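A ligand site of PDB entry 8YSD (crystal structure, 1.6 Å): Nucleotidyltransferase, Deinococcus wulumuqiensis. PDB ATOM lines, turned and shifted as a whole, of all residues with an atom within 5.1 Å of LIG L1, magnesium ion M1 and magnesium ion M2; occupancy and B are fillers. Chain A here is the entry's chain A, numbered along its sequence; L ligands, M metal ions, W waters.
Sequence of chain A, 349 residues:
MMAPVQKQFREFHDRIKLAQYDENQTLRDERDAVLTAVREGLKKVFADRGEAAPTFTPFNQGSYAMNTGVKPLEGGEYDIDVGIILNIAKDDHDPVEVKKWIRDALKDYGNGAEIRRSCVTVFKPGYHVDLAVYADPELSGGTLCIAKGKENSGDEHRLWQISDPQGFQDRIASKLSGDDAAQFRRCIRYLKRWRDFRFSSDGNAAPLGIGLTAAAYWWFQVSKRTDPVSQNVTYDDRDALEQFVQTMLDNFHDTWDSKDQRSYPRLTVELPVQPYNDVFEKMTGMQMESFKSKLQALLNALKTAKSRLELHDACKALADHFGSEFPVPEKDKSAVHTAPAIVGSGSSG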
ATOM      1  N   GLN A  61      22.742 -30.574 -23.209  1.00  0.00           N
ATOM      2  CA  GLN A  61      23.588 -29.433 -22.877  1.00  0.00           C
ATOM      3  C   GLN A  61      23.143 -28.794 -21.572  1.00  0.00           C
ATOM      4  O   GLN A  61      22.088 -29.132 -21.021  1.00  0.00           O
ATOM      5  CB  GLN A  61      23.569 -28.351 -23.975  1.00  0.00           C
ATOM      6  CG  GLN A  61      24.311 -28.768 -25.216  1.00  0.00           C
ATOM      7  CD  GLN A  61      24.734 -27.613 -26.085  1.00  0.00           C
ATOM      8  OE1 GLN A  61      24.362 -27.559 -27.250  1.00  0.00           O
ATOM      9  NE2 GLN A  61      25.563 -26.741 -25.558  1.00  0.00           N
ATOM     10  N   GLY A  62      23.966 -27.827 -21.094  1.00  0.00           N
ATOM     11  CA  GLY A  62      23.557 -26.952 -20.032  1.00  0.00           C
ATOM     12  C   GLY A  62      23.479 -27.638 -18.672  1.00  0.00           C
ATOM     13  O   GLY A  62      24.002 -28.748 -18.433  1.00  0.00           O
ATOM     14  N   SER A  63      22.801 -26.940 -17.768  1.00  0.00           N
ATOM     15  CA  SER A  63      22.824 -27.356 -16.383  1.00  0.00           C
ATOM     16  C   SER A  63      22.154 -28.716 -16.157  1.00  0.00           C
ATOM     17  O   SER A  63      22.543 -29.449 -15.244  1.00  0.00           O
ATOM     18  CB  SER A  63      22.168 -26.260 -15.552  1.00  0.00           C
ATOM     19  OG  SER A  63      20.769 -26.280 -15.789  1.00  0.00           O
ATOM     20  N   MET A  66      24.893 -31.120 -16.863  1.00  0.00           N
ATOM     21  CA  MET A  66      26.022 -31.014 -15.965  1.00  0.00           C
ATOM     22  C   MET A  66      25.617 -31.236 -14.506  1.00  0.00           C
ATOM     23  O   MET A  66      26.464 -31.104 -13.612  1.00  0.00           O
ATOM     24  CB  MET A  66      26.691 -29.641 -16.118  1.00  0.00           C
ATOM     25  CG  MET A  66      27.242 -29.370 -17.521  1.00  0.00           C
ATOM     26  SD  MET A  66      28.205 -27.891 -17.698  1.00  0.00           S
ATOM     27  CE  MET A  66      26.938 -26.603 -17.636  1.00  0.00           C
ATOM     28  N   THR A  68      23.870 -29.238 -12.588  1.00  0.00           N
ATOM     29  CA  THR A  68      23.917 -27.980 -11.855  1.00  0.00           C
ATOM     30  C   THR A  68      22.592 -27.222 -11.931  1.00  0.00           C
ATOM     31  O   THR A  68      22.539 -25.994 -11.732  1.00  0.00           O
ATOM     32  CB  THR A  68      25.014 -27.107 -12.427  1.00  0.00           C
ATOM     33  OG1 THR A  68      24.766 -26.961 -13.826  1.00  0.00           O
ATOM     34  CG2 THR A  68      26.388 -27.749 -12.222  1.00  0.00           C
ATOM     35  N   GLY A  69      21.490 -27.928 -12.137  1.00  0.00           N
ATOM     36  CA  GLY A  69      20.204 -27.286 -12.342  1.00  0.00           C
ATOM     37  C   GLY A  69      19.456 -26.928 -11.070  1.00  0.00           C
ATOM     38  O   GLY A  69      19.548 -27.620 -10.043  1.00  0.00           O
ATOM     39  N   ASP A  79      14.697 -24.334 -18.072  1.00  0.00           N
ATOM     40  CA  ASP A  79      15.495 -24.072 -19.243  1.00  0.00           C
ATOM     41  C   ASP A  79      16.098 -25.381 -19.748  1.00  0.00           C
ATOM     42  O   ASP A  79      17.135 -25.791 -19.243  1.00  0.00           O
ATOM     43  CB  ASP A  79      16.581 -23.097 -18.835  1.00  0.00           C
ATOM     44  CG  ASP A  79      17.467 -22.778 -19.923  1.00  0.00           C
ATOM     45  OD1 ASP A  79      16.911 -22.339 -20.937  1.00  0.00           O
ATOM     46  OD2 ASP A  79      18.670 -23.013 -19.806  1.00  0.00           O
ATOM     47  N   ASP A  81      18.254 -27.259 -22.180  1.00  0.00           N
ATOM     48  CA  ASP A  81      19.258 -26.947 -23.191  1.00  0.00           C
ATOM     49  C   ASP A  81      19.614 -28.218 -23.941  1.00  0.00           C
ATOM     50  O   ASP A  81      19.914 -29.239 -23.315  1.00  0.00           O
ATOM     51  CB  ASP A  81      20.520 -26.374 -22.541  1.00  0.00           C
ATOM     52  CG  ASP A  81      20.250 -25.113 -21.762  1.00  0.00           C
ATOM     53  OD1 ASP A  81      19.733 -24.159 -22.359  1.00  0.00           O
ATOM     54  OD2 ASP A  81      20.571 -25.069 -20.544  1.00  0.00           O
ATOM     55  N   HIS A 128      11.139 -23.387 -21.277  1.00  0.00           N
ATOM     56  CA  HIS A 128      11.486 -23.217 -22.669  1.00  0.00           C
ATOM     57  C   HIS A 128      12.597 -24.202 -22.992  1.00  0.00           C
ATOM     58  O   HIS A 128      13.294 -24.701 -22.107  1.00  0.00           O
ATOM     59  CB  HIS A 128      11.893 -21.786 -23.047  1.00  0.00           C
ATOM     60  CG  HIS A 128      12.995 -21.215 -22.217  1.00  0.00           C
ATOM     61  ND1 HIS A 128      12.770 -20.579 -21.011  1.00  0.00           N
ATOM     62  CD2 HIS A 128      14.336 -21.158 -22.426  1.00  0.00           C
ATOM     63  CE1 HIS A 128      13.919 -20.160 -20.519  1.00  0.00           C
ATOM     64  NE2 HIS A 128      14.884 -20.515 -21.345  1.00  0.00           N
ATOM     65  N   ASP A 130      15.949 -24.572 -25.324  1.00  0.00           N
ATOM     66  CA  ASP A 130      16.990 -23.824 -26.045  1.00  0.00           C
ATOM     67  C   ASP A 130      17.747 -24.847 -26.900  1.00  0.00           C
ATOM     68  O   ASP A 130      18.569 -25.607 -26.399  1.00  0.00           O
ATOM     69  CB  ASP A 130      17.954 -23.133 -25.080  1.00  0.00           C
ATOM     70  CG  ASP A 130      17.293 -22.028 -24.246  1.00  0.00           C
ATOM     71  OD1 ASP A 130      16.256 -21.498 -24.685  1.00  0.00           O
ATOM     72  OD2 ASP A 130      17.810 -21.712 -23.151  1.00  0.00           O
ATOM     73  N   PRO A 165      30.967 -27.785 -26.594  1.00  0.00           N
ATOM     74  CA  PRO A 165      30.113 -27.989 -25.401  1.00  0.00           C
ATOM     75  C   PRO A 165      30.435 -29.279 -24.666  1.00  0.00           C
ATOM     76  O   PRO A 165      30.371 -29.297 -23.425  1.00  0.00           O
ATOM     77  CB  PRO A 165      28.691 -27.985 -25.986  1.00  0.00           C
ATOM     78  CG  PRO A 165      28.879 -28.370 -27.421  1.00  0.00           C
ATOM     79  CD  PRO A 165      30.157 -27.702 -27.815  1.00  0.00           C
ATOM     80  N   PHE A 168      33.462 -28.643 -22.518  1.00  0.00           N
ATOM     81  CA  PHE A 168      33.096 -27.837 -21.348  1.00  0.00           C
ATOM     82  C   PHE A 168      32.387 -28.695 -20.302  1.00  0.00           C
ATOM     83  O   PHE A 168      32.711 -28.642 -19.110  1.00  0.00           O
ATOM     84  CB  PHE A 168      32.220 -26.630 -21.753  1.00  0.00           C
ATOM     85  CG  PHE A 168      31.808 -25.787 -20.589  1.00  0.00           C
ATOM     86  CD1 PHE A 168      32.742 -25.178 -19.792  1.00  0.00           C
ATOM     87  CD2 PHE A 168      30.465 -25.616 -20.282  1.00  0.00           C
ATOM     88  CE1 PHE A 168      32.376 -24.416 -18.668  1.00  0.00           C
ATOM     89  CE2 PHE A 168      30.083 -24.855 -19.183  1.00  0.00           C
ATOM     90  CZ  PHE A 168      31.023 -24.245 -18.378  1.00  0.00           C
ATOM     91  N   LYS A 192      22.962 -19.713  -8.242  1.00  0.00           N
ATOM     92  CA  LYS A 192      21.912 -19.536  -9.234  1.00  0.00           C
ATOM     93  C   LYS A 192      20.627 -19.098  -8.545  1.00  0.00           C
ATOM     94  O   LYS A 192      19.908 -18.251  -9.072  1.00  0.00           O
ATOM     95  CB  LYS A 192      21.695 -20.846 -10.018  1.00  0.00           C
ATOM     96  CG  LYS A 192      22.823 -21.075 -11.046  1.00  0.00           C
ATOM     97  CD  LYS A 192      22.602 -22.355 -11.782  1.00  0.00           C
ATOM     98  CE  LYS A 192      23.588 -22.587 -12.931  1.00  0.00           C
ATOM     99  NZ  LYS A 192      23.235 -23.885 -13.649  1.00  0.00           N
ATOM    100  N   ARG A 195      21.060 -15.495  -7.876  1.00  0.00           N
ATOM    101  CA  ARG A 195      20.758 -14.821  -9.134  1.00  0.00           C
ATOM    102  C   ARG A 195      19.264 -14.614  -9.283  1.00  0.00           C
ATOM    103  O   ARG A 195      18.797 -13.497  -9.597  1.00  0.00           O
ATOM    104  CB  ARG A 195      21.284 -15.647 -10.303  1.00  0.00           C
ATOM    105  CG  ARG A 195      20.912 -15.118 -11.712  1.00  0.00           C
ATOM    106  CD  ARG A 195      20.942 -16.270 -12.769  1.00  0.00           C
ATOM    107  NE  ARG A 195      20.047 -17.362 -12.430  1.00  0.00           N
ATOM    108  CZ  ARG A 195      20.094 -18.577 -12.987  1.00  0.00           C
ATOM    109  NH1 ARG A 195      21.023 -18.881 -13.889  1.00  0.00           N
ATOM    110  NH2 ARG A 195      19.227 -19.528 -12.602  1.00  0.00           N
ATOM    111  N   ALA A 206      20.944 -12.912 -17.572  1.00  0.00           N
ATOM    112  CA  ALA A 206      21.036 -14.151 -18.352  1.00  0.00           C
ATOM    113  C   ALA A 206      22.437 -14.756 -18.372  1.00  0.00           C
ATOM    114  O   ALA A 206      22.536 -15.992 -18.274  1.00  0.00           O
ATOM    115  CB  ALA A 206      20.536 -13.908 -19.779  1.00  0.00           C
ATOM    116  N   GLY A 209      24.168 -17.484 -15.103  1.00  0.00           N
ATOM    117  CA  GLY A 209      24.165 -18.929 -14.925  1.00  0.00           C
ATOM    118  C   GLY A 209      25.469 -19.597 -15.407  1.00  0.00           C
ATOM    119  O   GLY A 209      26.257 -20.171 -14.616  1.00  0.00           O
ATOM    120  N   ILE A 210      25.691 -19.485 -16.712  1.00  0.00           N
ATOM    121  CA  ILE A 210      26.934 -19.978 -17.296  1.00  0.00           C
ATOM    122  C   ILE A 210      28.139 -19.235 -16.726  1.00  0.00           C
ATOM    123  O   ILE A 210      29.182 -19.844 -16.443  1.00  0.00           O
ATOM    124  CB  ILE A 210      26.880 -19.895 -18.836  1.00  0.00           C
ATOM    125  CG1 ILE A 210      28.174 -20.400 -19.442  1.00  0.00           C
ATOM    126  CG2 ILE A 210      26.688 -18.457 -19.292  1.00  0.00           C
ATOM    127  CD1 ILE A 210      28.510 -21.805 -19.072  1.00  0.00           C
ATOM    128  N   THR A 213      28.986 -20.631 -13.439  1.00  0.00           N
ATOM    129  CA  THR A 213      29.513 -21.988 -13.577  1.00  0.00           C
ATOM    130  C   THR A 213      30.966 -21.944 -14.006  1.00  0.00           C
ATOM    131  O   THR A 213      31.817 -22.653 -13.431  1.00  0.00           O
ATOM    132  CB  THR A 213      28.668 -22.783 -14.569  1.00  0.00           C
ATOM    133  OG1 THR A 213      27.312 -22.764 -14.099  1.00  0.00           O
ATOM    134  CG2 THR A 213      29.124 -24.264 -14.735  1.00  0.00           C
ATOM    135  N   LEU A 271      35.658 -18.881 -21.035  1.00  0.00           N
ATOM    136  CA  LEU A 271      35.297 -20.296 -21.160  1.00  0.00           C
ATOM    137  C   LEU A 271      36.589 -21.105 -21.205  1.00  0.00           C
ATOM    138  O   LEU A 271      37.524 -20.714 -21.907  1.00  0.00           O
ATOM    139  CB  LEU A 271      34.509 -20.525 -22.439  1.00  0.00           C
ATOM    140  CG  LEU A 271      33.671 -21.795 -22.492  1.00  0.00           C
ATOM    141  CD1 LEU A 271      32.462 -21.695 -21.571  1.00  0.00           C
ATOM    142  CD2 LEU A 271      33.172 -22.011 -23.919  1.00  0.00           C
ATOM    143  N   ASN A 277      35.706 -17.618 -25.150  1.00  0.00           N
ATOM    144  CA  ASN A 277      35.119 -16.280 -25.055  1.00  0.00           C
ATOM    145  C   ASN A 277      34.852 -15.908 -23.602  1.00  0.00           C
ATOM    146  O   ASN A 277      34.652 -16.784 -22.754  1.00  0.00           O
ATOM    147  CB  ASN A 277      33.811 -16.235 -25.841  1.00  0.00           C
ATOM    148  CG  ASN A 277      32.780 -17.218 -25.295  1.00  0.00           C
ATOM    149  OD1 ASN A 277      32.973 -18.452 -25.345  1.00  0.00           O
ATOM    150  ND2 ASN A 277      31.692 -16.687 -24.757  1.00  0.00           N
ATOM    151  N   VAL A 279      32.545 -15.226 -20.955  1.00  0.00           N
ATOM    152  CA  VAL A 279      31.126 -15.513 -20.897  1.00  0.00           C
ATOM    153  C   VAL A 279      30.323 -14.366 -20.296  1.00  0.00           C
ATOM    154  O   VAL A 279      29.096 -14.375 -20.384  1.00  0.00           O
ATOM    155  CB  VAL A 279      30.888 -16.815 -20.109  1.00  0.00           C
ATOM    156  CG1 VAL A 279      31.551 -17.993 -20.855  1.00  0.00           C
ATOM    157  CG2 VAL A 279      31.423 -16.676 -18.714  1.00  0.00           C
HETATM  158  P1  LIG L   1      21.367 -22.259 -16.221  1.00  0.00           P
HETATM  159  O1  LIG L   1      21.481 -20.846 -15.795  1.00  0.00           O
HETATM  160  O2  LIG L   1      20.552 -22.428 -17.473  1.00  0.00           O
HETATM  161  O3  LIG L   1      21.037 -23.224 -15.122  1.00  0.00           O
HETATM  162  P2  LIG L   1      23.325 -23.284 -17.985  1.00  0.00           P
HETATM  163  O4  LIG L   1      24.723 -23.842 -17.897  1.00  0.00           O
HETATM  164  O5  LIG L   1      22.280 -24.246 -18.482  1.00  0.00           O
HETATM  165  O6  LIG L   1      22.909 -22.589 -16.618  1.00  0.00           O
HETATM  166  P3  LIG L   1      22.587 -21.602 -20.333  1.00  0.00           P
HETATM  167  O7  LIG L   1      22.658 -20.106 -20.403  1.00  0.00           O
HETATM  168  O8  LIG L   1      21.264 -22.278 -20.332  1.00  0.00           O
HETATM  169  O9  LIG L   1      23.466 -22.070 -19.041  1.00  0.00           O
HETATM  170  O10 LIG L   1      23.436 -22.156 -21.591  1.00  0.00           O
HETATM  171  C1  LIG L   1      23.408 -23.530 -21.956  1.00  0.00           C
HETATM  172  C2  LIG L   1      24.852 -23.951 -22.305  1.00  0.00           C
HETATM  173  O11 LIG L   1      25.237 -23.160 -23.431  1.00  0.00           O
HETATM  174  C3  LIG L   1      25.914 -23.615 -21.277  1.00  0.00           C
HETATM  175  O12 LIG L   1      26.065 -24.633 -20.272  1.00  0.00           O
HETATM  176  C4  LIG L   1      27.170 -23.514 -22.121  1.00  0.00           C
HETATM  177  O13 LIG L   1      27.626 -24.834 -22.501  1.00  0.00           O
HETATM  178  C5  LIG L   1      26.628 -22.833 -23.363  1.00  0.00           C
HETATM  179  N1  LIG L   1      26.744 -21.375 -23.231  1.00  0.00           N
HETATM  180  C6  LIG L   1      25.750 -20.527 -22.871  1.00  0.00           C
HETATM  181  N2  LIG L   1      26.170 -19.248 -22.887  1.00  0.00           N
HETATM  182  C7  LIG L   1      27.449 -19.254 -23.268  1.00  0.00           C
HETATM  183  C8  LIG L   1      28.464 -18.210 -23.469  1.00  0.00           C
HETATM  184  N3  LIG L   1      28.215 -16.894 -23.288  1.00  0.00           N
HETATM  185  N4  LIG L   1      29.654 -18.665 -23.886  1.00  0.00           N
HETATM  186  C9  LIG L   1      29.912 -19.967 -24.098  1.00  0.00           C
HETATM  187  N5  LIG L   1      29.046 -20.960 -23.917  1.00  0.00           N
HETATM  188  C10 LIG L   1      27.816 -20.653 -23.512  1.00  0.00           C
HETATM  189  P1  LG2 L   2      21.681 -10.734 -27.859  1.00  0.00           P
HETATM  190  O1  LG2 L   2      21.266 -10.665 -26.409  1.00  0.00           O
HETATM  191  O2  LG2 L   2      23.184 -10.761 -28.052  1.00  0.00           O
HETATM  192  O3  LG2 L   2      20.972  -9.782 -28.785  1.00  0.00           O
HETATM  193  P2  LG2 L   2      20.201 -13.130 -27.560  1.00  0.00           P
HETATM  194  O4  LG2 L   2      19.165 -12.308 -26.844  1.00  0.00           O
HETATM  195  O5  LG2 L   2      19.732 -14.226 -28.487  1.00  0.00           O
HETATM  196  O6  LG2 L   2      21.244 -12.206 -28.353  1.00  0.00           O
HETATM  197  P3  LG2 L   2      22.412 -14.766 -26.718  1.00  0.00           P
HETATM  198  O7  LG2 L   2      23.324 -14.695 -25.514  1.00  0.00           O
HETATM  199  O8  LG2 L   2      23.028 -14.556 -28.077  1.00  0.00           O
HETATM  200  O9  LG2 L   2      21.171 -13.766 -26.441  1.00  0.00           O
HETATM  201  O10 LG2 L   2      21.655 -16.182 -26.732  1.00  0.00           O
HETATM  202  C1  LG2 L   2      20.534 -16.346 -25.868  1.00  0.00           C
HETATM  203  C2  LG2 L   2      20.560 -17.701 -25.171  1.00  0.00           C
HETATM  204  O11 LG2 L   2      21.504 -18.537 -25.848  1.00  0.00           O
HETATM  205  C3  LG2 L   2      21.014 -17.539 -23.722  1.00  0.00           C
HETATM  206  O12 LG2 L   2      20.314 -18.470 -22.883  1.00  0.00           O
HETATM  207  C4  LG2 L   2      22.464 -17.947 -23.726  1.00  0.00           C
HETATM  208  O13 LG2 L   2      22.863 -18.539 -22.489  1.00  0.00           O
HETATM  209  C5  LG2 L   2      22.510 -18.925 -24.900  1.00  0.00           C
HETATM  210  N1  LG2 L   2      23.895 -18.962 -25.449  1.00  0.00           N
HETATM  211  C6  LG2 L   2      24.768 -17.943 -25.551  1.00  0.00           C
HETATM  212  N2  LG2 L   2      25.940 -18.353 -26.067  1.00  0.00           N
HETATM  213  C7  LG2 L   2      25.834 -19.669 -26.298  1.00  0.00           C
HETATM  214  C8  LG2 L   2      26.703 -20.712 -26.817  1.00  0.00           C
HETATM  215  N3  LG2 L   2      27.960 -20.428 -27.224  1.00  0.00           N
HETATM  216  N4  LG2 L   2      26.191 -21.954 -26.850  1.00  0.00           N
HETATM  217  C9  LG2 L   2      24.942 -22.265 -26.459  1.00  0.00           C
HETATM  218  N5  LG2 L   2      24.089 -21.350 -25.993  1.00  0.00           N
HETATM  219  C10 LG2 L   2      24.480 -20.071 -25.868  1.00  0.00           C
HETATM  220 MG    MG M   1      20.401 -23.695 -19.005  1.00  0.00          MG
HETATM  221 MG    MG M   2      19.394 -22.146 -21.769  1.00  0.00          MG
HETATM  222  O   HOH W   1      20.548 -21.598 -23.208  1.00  0.00           O
HETATM  223  O   HOH W   2      26.405 -27.307 -22.567  1.00  0.00           O
HETATM  224  O   HOH W   3      23.303 -18.851 -18.237  1.00  0.00           O
HETATM  225  O   HOH W   4      19.469 -25.217 -18.025  1.00  0.00           O
HETATM  226  O   HOH W   5      19.159 -24.614 -13.969  1.00  0.00           O
HETATM  227  O   HOH W   6      31.040 -19.471 -26.858  1.00  0.00           O
HETATM  228  O   HOH W   7      18.956 -21.587 -13.950  1.00  0.00           O
HETATM  229  O   HOH W   8      25.455 -24.478 -15.215  1.00  0.00           O
HETATM  230  O   HOH W   9      29.526 -24.120 -24.660  1.00  0.00           O
HETATM  231  O   HOH W  10      18.905 -20.305 -20.923  1.00  0.00           O
HETATM  232  O   HOH W  11      19.268 -20.068 -18.051  1.00  0.00           O
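An oxygen (O3) of LIG L1 is in salt-bridge range of the side-chain amino group (NZ) of Lys 192 (2.7 Å). NH1 of Arg 195 lies within salt-bridge range of O1 of LIG L1, 2.8 Å away. The backbone NH (N) of Ser 63 lies close to an oxygen (O5) of LIG L1, 2.8 Å away. O3 of LIG L1 is in hydrogen-bond range of OG of Ser 63, 3.1 Å away. ND2 of Asn 277 lies within hydrogen-bond range of N4 of LIG L1 (3.0 Å).
An oxygen (O13) of LG2 L2 lies within hydrogen-bond range of an oxygen (O7) of LIG L1 (2.6 Å).
A ring nitrogen (NE2) of His 128 is in hydrogen-bond range of the side-chain carboxylate (OD1) of Asp 79, at 2.8 Å. N of Gln 61 lies within hydrogen-bond range of O of Asp 81 (3.1 Å). The guanidinium group (NE) of Arg 195 sits close to the backbone carbonyl oxygen (O) of Lys 192, 3.5 Å away. The side-chain amino group of Lys 192 lies within hydrogen-bond range of the backbone carbonyl oxygen of Thr 68, 2.9 Å away. The backbone carbonyl oxygen of Ser 63 lies within hydrogen-bond range of the backbone NH of Thr 68 (3.0 Å). The backbone NH of Leu 271 is in hydrogen-bond range of the backbone carbonyl oxygen of Asn 277 (2.9 Å). OG1 of Thr 213 is in hydrogen-bond range of O of Gly 209, at 2.8 Å.
Gly 62 touches LIG L1. Met 66 touches LIG L1. Phe 168 touches LIG L1. Gly 209 touches LIG L1 (CA to O1, 3.4 Å). Ile 210 touches LIG L1 (CG2 to N2, 3.7 Å). CD2 of Leu 271 touches C9 of LIG L1, at 3.9 Å. Val 279 touches LIG L1 (CG1 to N4, 3.6 Å). Hydrophobic or aromatic side chains within 4 Å of LIG L1: Met 66, Phe 168, Ile 210, Leu 271 and Val 279. Of the 21 residues printed, 13 come within 4 Å of LIG L1.
Two residues have an atom within 4 Å of magnesium ion M1: Asp 79 and Asp 81. The nearest printed residue that does not touch magnesium ion M1 is Ser 63 (4.1 Å).
Within 4 Å of magnesium ion M2: Asp 79, Asp 81 and Asp 130. The nearest printed residue that does not touch magnesium ion M2 is His 128 (4.8 Å).
Magnesium ion M1 is bound by O2 of LIG L1 (2.0 Å), OD2 of Asp 79 (2.0 Å), O5 of LIG L1 (2.0 Å), water W4 (2.0 Å), OD2 of Asp 81 (2.1 Å) and O8 of LIG L1 (2.1 Å).
Magnesium ion M2 is bound by water W1 (1.9 Å), water W10 (2.1 Å), OD1 of Asp 81 (2.1 Å), OD2 of Asp 130 (2.1 Å), OD2 of Asp 79 (2.3 Å) and O8 of LIG L1 (2.4 Å). Slightly farther from magnesium ion M2 lies OD1 of Asp 79 (2.6 Å).
Water W4 bridges O of Asp 79 (2.7 Å) and OG of Ser 63 (2.8 Å). Water W10 bridges OD1 of Asp 79 and O12 of LG2 L2. Water W1 bridges an oxygen (O12) of LG2 L2 (3.2 Å) and an oxygen (O10) of LIG L1 (3.4 Å). Water W5 bridges O3 of LIG L1 (2.6 Å) and OG of Ser 63 (2.9 Å). Water W7 bridges NH2 of Arg 195 (2.5 Å) and O3 of LIG L1 (2.9 Å). Water W6 lies within hydrogen-bond range of the side-chain amide oxygen (OD1) of Asn 277 (2.7 Å), a nitrogen (N3) of LG2 L2 (3.2 Å) and a nitrogen (N4) of LIG L1 (3.4 Å).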
